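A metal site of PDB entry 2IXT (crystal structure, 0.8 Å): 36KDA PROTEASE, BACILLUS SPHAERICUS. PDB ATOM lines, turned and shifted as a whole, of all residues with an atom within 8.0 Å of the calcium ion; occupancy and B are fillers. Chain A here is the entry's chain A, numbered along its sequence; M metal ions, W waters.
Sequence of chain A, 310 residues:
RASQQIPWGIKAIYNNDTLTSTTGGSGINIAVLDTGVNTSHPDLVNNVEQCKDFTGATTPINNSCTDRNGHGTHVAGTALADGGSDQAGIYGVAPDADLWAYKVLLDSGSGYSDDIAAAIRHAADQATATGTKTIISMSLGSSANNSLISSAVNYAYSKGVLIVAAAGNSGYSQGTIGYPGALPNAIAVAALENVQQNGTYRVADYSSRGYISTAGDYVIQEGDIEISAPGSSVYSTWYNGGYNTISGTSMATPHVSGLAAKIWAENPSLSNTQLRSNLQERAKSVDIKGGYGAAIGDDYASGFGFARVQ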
ATOM      1  N   THR A 200      -4.309  -7.096 -26.015  1.00  0.00           N
ATOM      2  CA  THR A 200      -4.285  -8.216 -26.911  1.00  0.00           C
ATOM      3  C   THR A 200      -4.135  -7.723 -28.335  1.00  0.00           C
ATOM      4  O   THR A 200      -4.311  -6.528 -28.621  1.00  0.00           O
ATOM      5  CB  THR A 200      -5.547  -9.095 -26.812  1.00  0.00           C
ATOM      6  OG1 THR A 200      -6.659  -8.511 -27.489  1.00  0.00           O
ATOM      7  CG2 THR A 200      -5.964  -9.350 -25.371  1.00  0.00           C
ATOM      8  N   VAL A 203      -8.738  -7.092 -33.489  1.00  0.00           N
ATOM      9  CA  VAL A 203      -9.433  -7.527 -34.690  1.00  0.00           C
ATOM     10  C   VAL A 203      -9.466  -6.352 -35.683  1.00  0.00           C
ATOM     11  O   VAL A 203      -9.768  -5.201 -35.307  1.00  0.00           O
ATOM     12  CB  VAL A 203     -10.864  -7.952 -34.345  1.00  0.00           C
ATOM     13  CG1 VAL A 203     -11.627  -8.385 -35.591  1.00  0.00           C
ATOM     14  CG2 VAL A 203     -10.881  -9.066 -33.319  1.00  0.00           C
ATOM     15  N   TYR A 218     -18.873 -20.346 -25.847  1.00  0.00           N
ATOM     16  CA  TYR A 218     -17.822 -21.259 -26.296  1.00  0.00           C
ATOM     17  C   TYR A 218     -18.378 -22.555 -26.914  1.00  0.00           C
ATOM     18  O   TYR A 218     -17.762 -23.596 -26.814  1.00  0.00           O
ATOM     19  CB  TYR A 218     -16.776 -21.575 -25.208  1.00  0.00           C
ATOM     20  CG  TYR A 218     -15.910 -20.410 -24.785  1.00  0.00           C
ATOM     21  CD1 TYR A 218     -16.185 -19.696 -23.643  1.00  0.00           C
ATOM     22  CD2 TYR A 218     -14.817 -20.037 -25.519  1.00  0.00           C
ATOM     23  CE1 TYR A 218     -15.359 -18.677 -23.193  1.00  0.00           C
ATOM     24  CE2 TYR A 218     -13.965 -19.003 -25.119  1.00  0.00           C
ATOM     25  CZ  TYR A 218     -14.246 -18.333 -23.935  1.00  0.00           C
ATOM     26  OH  TYR A 218     -13.401 -17.351 -23.455  1.00  0.00           O
ATOM     27  N   SER A 228      -9.499 -16.423 -34.278  1.00  0.00           N
ATOM     28  CA  SER A 228      -8.847 -15.268 -34.878  1.00  0.00           C
ATOM     29  C   SER A 228      -7.409 -15.612 -35.258  1.00  0.00           C
ATOM     30  O   SER A 228      -6.747 -16.388 -34.574  1.00  0.00           O
ATOM     31  CB  SER A 228      -8.848 -14.137 -33.880  1.00  0.00           C
ATOM     32  OG  SER A 228     -10.159 -13.664 -33.590  1.00  0.00           O
ATOM     33  N   ALA A 283      -7.487 -21.562 -28.802  1.00  0.00           N
ATOM     34  CA  ALA A 283      -8.007 -20.197 -28.950  1.00  0.00           C
ATOM     35  C   ALA A 283      -8.544 -19.656 -27.665  1.00  0.00           C
ATOM     36  O   ALA A 283      -8.271 -18.503 -27.307  1.00  0.00           O
ATOM     37  CB  ALA A 283      -9.099 -20.184 -30.022  1.00  0.00           C
ATOM     38  N   LYS A 284      -9.302 -20.458 -26.917  1.00  0.00           N
ATOM     39  CA  LYS A 284      -9.888 -20.010 -25.682  1.00  0.00           C
ATOM     40  C   LYS A 284      -8.818 -19.498 -24.727  1.00  0.00           C
ATOM     41  O   LYS A 284      -9.064 -18.553 -23.940  1.00  0.00           O
ATOM     42  CB  LYS A 284     -10.722 -21.122 -25.060  1.00  0.00           C
ATOM     43  CG  LYS A 284     -11.288 -20.793 -23.720  1.00  0.00           C
ATOM     44  CD  LYS A 284     -12.253 -21.865 -23.271  1.00  0.00           C
ATOM     45  CE  LYS A 284     -12.918 -21.559 -21.954  1.00  0.00           C
ATOM     46  NZ  LYS A 284     -13.733 -22.693 -21.375  1.00  0.00           N
ATOM     47  N   VAL A 286      -6.202 -17.870 -25.323  1.00  0.00           N
ATOM     48  CA  VAL A 286      -5.638 -16.571 -25.741  1.00  0.00           C
ATOM     49  C   VAL A 286      -6.828 -15.683 -26.133  1.00  0.00           C
ATOM     50  O   VAL A 286      -7.197 -15.535 -27.283  1.00  0.00           O
ATOM     51  CB  VAL A 286      -4.624 -16.711 -26.892  1.00  0.00           C
ATOM     52  CG1 VAL A 286      -4.002 -15.380 -27.178  1.00  0.00           C
ATOM     53  CG2 VAL A 286      -3.563 -17.770 -26.547  1.00  0.00           C
ATOM     54  N   ASP A 287      -7.440 -15.094 -25.099  1.00  0.00           N
ATOM     55  CA  ASP A 287      -8.645 -14.272 -25.290  1.00  0.00           C
ATOM     56  C   ASP A 287      -8.273 -12.991 -26.027  1.00  0.00           C
ATOM     57  O   ASP A 287      -7.318 -12.337 -25.682  1.00  0.00           O
ATOM     58  CB  ASP A 287      -9.215 -13.971 -23.904  1.00  0.00           C
ATOM     59  CG  ASP A 287     -10.539 -13.267 -23.900  1.00  0.00           C
ATOM     60  OD1 ASP A 287     -11.080 -12.998 -24.985  1.00  0.00           O
ATOM     61  OD2 ASP A 287     -11.027 -12.975 -22.769  1.00  0.00           O
ATOM     62  N   ILE A 288      -8.974 -12.691 -27.122  1.00  0.00           N
ATOM     63  CA  ILE A 288      -8.810 -11.447 -27.846  1.00  0.00           C
ATOM     64  C   ILE A 288      -9.841 -10.441 -27.311  1.00  0.00           C
ATOM     65  O   ILE A 288     -11.043 -10.767 -27.188  1.00  0.00           O
ATOM     66  CB  ILE A 288      -8.963 -11.670 -29.339  1.00  0.00           C
ATOM     67  CG1 ILE A 288      -7.799 -12.526 -29.867  1.00  0.00           C
ATOM     68  CG2 ILE A 288      -9.107 -10.365 -30.085  1.00  0.00           C
ATOM     69  CD1 ILE A 288      -6.423 -11.859 -29.788  1.00  0.00           C
ATOM     70  N   LYS A 289      -9.377  -9.228 -27.013  1.00  0.00           N
ATOM     71  CA  LYS A 289     -10.174  -8.197 -26.372  1.00  0.00           C
ATOM     72  C   LYS A 289     -10.159  -6.882 -27.154  1.00  0.00           C
ATOM     73  O   LYS A 289     -10.796  -5.913 -26.706  1.00  0.00           O
ATOM     74  CB  LYS A 289      -9.689  -7.955 -24.953  1.00  0.00           C
ATOM     75  CG  LYS A 289      -9.824  -9.168 -24.032  1.00  0.00           C
ATOM     76  CD  LYS A 289      -9.147  -8.914 -22.728  1.00  0.00           C
ATOM     77  CE  LYS A 289      -9.305 -10.002 -21.721  1.00  0.00           C
ATOM     78  NZ  LYS A 289      -8.389  -9.807 -20.547  1.00  0.00           N
ATOM     79  N   GLY A 290      -9.428  -6.810 -28.268  1.00  0.00           N
ATOM     80  CA  GLY A 290      -9.283  -5.560 -29.012  1.00  0.00           C
ATOM     81  C   GLY A 290     -10.103  -5.578 -30.294  1.00  0.00           C
ATOM     82  O   GLY A 290     -10.162  -6.608 -30.981  1.00  0.00           O
ATOM     83  N   GLY A 293     -16.578  -4.755 -30.833  1.00  0.00           N
ATOM     84  CA  GLY A 293     -17.303  -5.950 -30.433  1.00  0.00           C
ATOM     85  C   GLY A 293     -16.489  -6.941 -29.626  1.00  0.00           C
ATOM     86  O   GLY A 293     -17.065  -7.857 -29.029  1.00  0.00           O
ATOM     87  N   ALA A 294     -15.166  -6.791 -29.575  1.00  0.00           N
ATOM     88  CA  ALA A 294     -14.353  -7.701 -28.813  1.00  0.00           C
ATOM     89  C   ALA A 294     -14.543  -7.493 -27.333  1.00  0.00           C
ATOM     90  O   ALA A 294     -14.738  -6.363 -26.864  1.00  0.00           O
ATOM     91  CB  ALA A 294     -12.876  -7.591 -29.220  1.00  0.00           C
ATOM     92  N   ALA A 295     -14.473  -8.564 -26.580  1.00  0.00           N
ATOM     93  CA  ALA A 295     -14.853  -8.561 -25.159  1.00  0.00           C
ATOM     94  C   ALA A 295     -14.077  -9.605 -24.420  1.00  0.00           C
ATOM     95  O   ALA A 295     -13.464 -10.522 -25.018  1.00  0.00           O
ATOM     96  CB  ALA A 295     -16.342  -8.887 -25.057  1.00  0.00           C
ATOM     97  N   ILE A 296     -14.102  -9.538 -23.102  1.00  0.00           N
ATOM     98  CA  ILE A 296     -13.652 -10.646 -22.297  1.00  0.00           C
ATOM     99  C   ILE A 296     -14.472 -11.914 -22.695  1.00  0.00           C
ATOM    100  O   ILE A 296     -15.698 -11.854 -22.785  1.00  0.00           O
ATOM    101  CB  ILE A 296     -13.800 -10.325 -20.833  1.00  0.00           C
ATOM    102  CG1 ILE A 296     -12.945  -9.078 -20.435  1.00  0.00           C
ATOM    103  CG2 ILE A 296     -13.471 -11.502 -19.976  1.00  0.00           C
ATOM    104  CD1 ILE A 296     -13.317  -8.460 -19.064  1.00  0.00           C
ATOM    105  N   GLY A 297     -13.782 -13.017 -22.924  1.00  0.00           N
ATOM    106  CA  GLY A 297     -14.401 -14.269 -23.266  1.00  0.00           C
ATOM    107  C   GLY A 297     -14.715 -14.422 -24.738  1.00  0.00           C
ATOM    108  O   GLY A 297     -14.183 -13.724 -25.620  1.00  0.00           O
ATOM    109  N   ASP A 298     -15.592 -15.382 -25.064  1.00  0.00           N
ATOM    110  CA  ASP A 298     -15.996 -15.667 -26.442  1.00  0.00           C
ATOM    111  C   ASP A 298     -16.847 -14.513 -26.933  1.00  0.00           C
ATOM    112  O   ASP A 298     -17.832 -14.174 -26.264  1.00  0.00           O
ATOM    113  CB  ASP A 298     -16.787 -16.987 -26.400  1.00  0.00           C
ATOM    114  CG  ASP A 298     -17.494 -17.348 -27.666  1.00  0.00           C
ATOM    115  OD1 ASP A 298     -18.541 -18.065 -27.561  1.00  0.00           O
ATOM    116  OD2 ASP A 298     -17.018 -16.940 -28.746  1.00  0.00           O
ATOM    117  N   ASP A 299     -16.489 -13.936 -28.072  1.00  0.00           N
ATOM    118  CA  ASP A 299     -17.221 -12.763 -28.550  1.00  0.00           C
ATOM    119  C   ASP A 299     -17.397 -12.805 -30.029  1.00  0.00           C
ATOM    120  O   ASP A 299     -16.794 -13.628 -30.748  1.00  0.00           O
ATOM    121  CB  ASP A 299     -16.533 -11.473 -28.055  1.00  0.00           C
ATOM    122  CG  ASP A 299     -15.161 -11.283 -28.656  1.00  0.00           C
ATOM    123  OD1 ASP A 299     -14.154 -11.277 -27.913  1.00  0.00           O
ATOM    124  OD2 ASP A 299     -15.068 -11.125 -29.914  1.00  0.00           O
ATOM    125  N   TYR A 300     -18.253 -11.921 -30.553  1.00  0.00           N
ATOM    126  CA  TYR A 300     -18.652 -11.976 -31.958  1.00  0.00           C
ATOM    127  C   TYR A 300     -17.684 -11.282 -32.900  1.00  0.00           C
ATOM    128  O   TYR A 300     -17.880 -11.328 -34.136  1.00  0.00           O
ATOM    129  CB  TYR A 300     -20.065 -11.541 -32.242  1.00  0.00           C
ATOM    130  CG  TYR A 300     -20.316 -10.150 -31.786  1.00  0.00           C
ATOM    131  CD1 TYR A 300     -20.019  -9.081 -32.613  1.00  0.00           C
ATOM    132  CD2 TYR A 300     -20.760  -9.922 -30.508  1.00  0.00           C
ATOM    133  CE1 TYR A 300     -20.186  -7.788 -32.193  1.00  0.00           C
ATOM    134  CE2 TYR A 300     -20.948  -8.617 -30.056  1.00  0.00           C
ATOM    135  CZ  TYR A 300     -20.671  -7.559 -30.907  1.00  0.00           C
ATOM    136  OH  TYR A 300     -20.861  -6.255 -30.531  1.00  0.00           O
ATOM    137  N   ALA A 301     -16.617 -10.671 -32.366  1.00  0.00           N
ATOM    138  CA  ALA A 301     -15.554 -10.103 -33.224  1.00  0.00           C
ATOM    139  C   ALA A 301     -14.431 -11.114 -33.463  1.00  0.00           C
ATOM    140  O   ALA A 301     -13.878 -11.183 -34.581  1.00  0.00           O
ATOM    141  CB  ALA A 301     -14.969  -8.863 -32.599  1.00  0.00           C
ATOM    142  N   SER A 302     -14.069 -11.859 -32.425  1.00  0.00           N
ATOM    143  CA  SER A 302     -12.854 -12.657 -32.424  1.00  0.00           C
ATOM    144  C   SER A 302     -13.113 -14.123 -32.118  1.00  0.00           C
ATOM    145  O   SER A 302     -12.186 -14.938 -32.112  1.00  0.00           O
ATOM    146  CB  SER A 302     -11.863 -12.076 -31.436  1.00  0.00           C
ATOM    147  OG  SER A 302     -12.309 -12.142 -30.111  1.00  0.00           O
ATOM    148  N   GLY A 303     -14.368 -14.480 -31.838  1.00  0.00           N
ATOM    149  CA  GLY A 303     -14.677 -15.837 -31.474  1.00  0.00           C
ATOM    150  C   GLY A 303     -14.010 -16.231 -30.158  1.00  0.00           C
ATOM    151  O   GLY A 303     -14.004 -15.462 -29.161  1.00  0.00           O
ATOM    152  N   PHE A 304     -13.521 -17.450 -30.097  1.00  0.00           N
ATOM    153  CA  PHE A 304     -12.977 -17.987 -28.874  1.00  0.00           C
ATOM    154  C   PHE A 304     -11.668 -17.327 -28.500  1.00  0.00           C
ATOM    155  O   PHE A 304     -11.323 -17.342 -27.301  1.00  0.00           O
ATOM    156  CB  PHE A 304     -12.784 -19.502 -29.018  1.00  0.00           C
ATOM    157  CG  PHE A 304     -14.047 -20.325 -29.098  1.00  0.00           C
ATOM    158  CD1 PHE A 304     -15.313 -19.806 -29.376  1.00  0.00           C
ATOM    159  CD2 PHE A 304     -13.941 -21.697 -28.924  1.00  0.00           C
ATOM    160  CE1 PHE A 304     -16.423 -20.631 -29.519  1.00  0.00           C
ATOM    161  CE2 PHE A 304     -15.065 -22.531 -28.997  1.00  0.00           C
ATOM    162  CZ  PHE A 304     -16.297 -21.991 -29.350  1.00  0.00           C
ATOM    163  N   GLY A 305     -10.930 -16.828 -29.481  1.00  0.00           N
ATOM    164  CA  GLY A 305      -9.616 -16.246 -29.242  1.00  0.00           C
ATOM    165  C   GLY A 305      -8.656 -16.572 -30.364  1.00  0.00           C
ATOM    166  O   GLY A 305      -9.085 -16.889 -31.483  1.00  0.00           O
ATOM    167  N   PHE A 306      -7.365 -16.458 -30.059  1.00  0.00           N
ATOM    168  CA  PHE A 306      -6.275 -16.589 -31.031  1.00  0.00           C
ATOM    169  C   PHE A 306      -5.536 -17.887 -30.742  1.00  0.00           C
ATOM    170  O   PHE A 306      -4.728 -17.963 -29.809  1.00  0.00           O
ATOM    171  CB  PHE A 306      -5.370 -15.377 -30.865  1.00  0.00           C
ATOM    172  CG  PHE A 306      -4.130 -15.359 -31.727  1.00  0.00           C
ATOM    173  CD1 PHE A 306      -3.068 -14.530 -31.372  1.00  0.00           C
ATOM    174  CD2 PHE A 306      -3.994 -16.111 -32.870  1.00  0.00           C
ATOM    175  CE1 PHE A 306      -1.945 -14.423 -32.141  1.00  0.00           C
ATOM    176  CE2 PHE A 306      -2.836 -16.034 -33.649  1.00  0.00           C
ATOM    177  CZ  PHE A 306      -1.816 -15.181 -33.288  1.00  0.00           C
HETATM  178 CA    CA M   1     -12.681 -12.183 -26.373  1.00  0.00          CA
HETATM  179  O   HOH W   1     -11.980 -13.758 -28.013  1.00  0.00           O
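The side-chain hydroxyl of Ser 302 sits close to the backbone carbonyl oxygen of Ile 288 (3.5 Å).
OD2 of Asp 299 lies within hydrogen-bond range of N of Ser 302 (2.8 Å).
OD2 of Asp 299 sits at hydrogen-bond distance from N of Ala 301, 2.9 Å away.
The side-chain hydroxyl (OG) of Ser 228 lies within hydrogen-bond range of the backbone carbonyl oxygen (O) of Ser 302 (2.8 Å).
Water W1 lies within hydrogen-bond range of OG of Ser 302 (2.7 Å), O of Gly 303 (2.9 Å) and N of Ile 288 (3.3 Å).
The calcium ion is bound by OD1 of Asp 287 (2.3 Å), O of Gly 297 (2.3 Å), O of Ala 295 (2.3 Å), O of Ile 288 (2.3 Å), OD1 of Asp 299 (2.3 Å) and water W1 (2.4 Å).
Ser 302 touches the calcium ion (OG to CA, 3.8 Å).
Six residues have an atom within 4 Å of the calcium ion: Asp 287, Ile 288, Ala 295, Gly 297, Asp 299 and Ser 302.
The nearest printed residue that does not touch the calcium ion is Ile 296 (4.1 Å).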
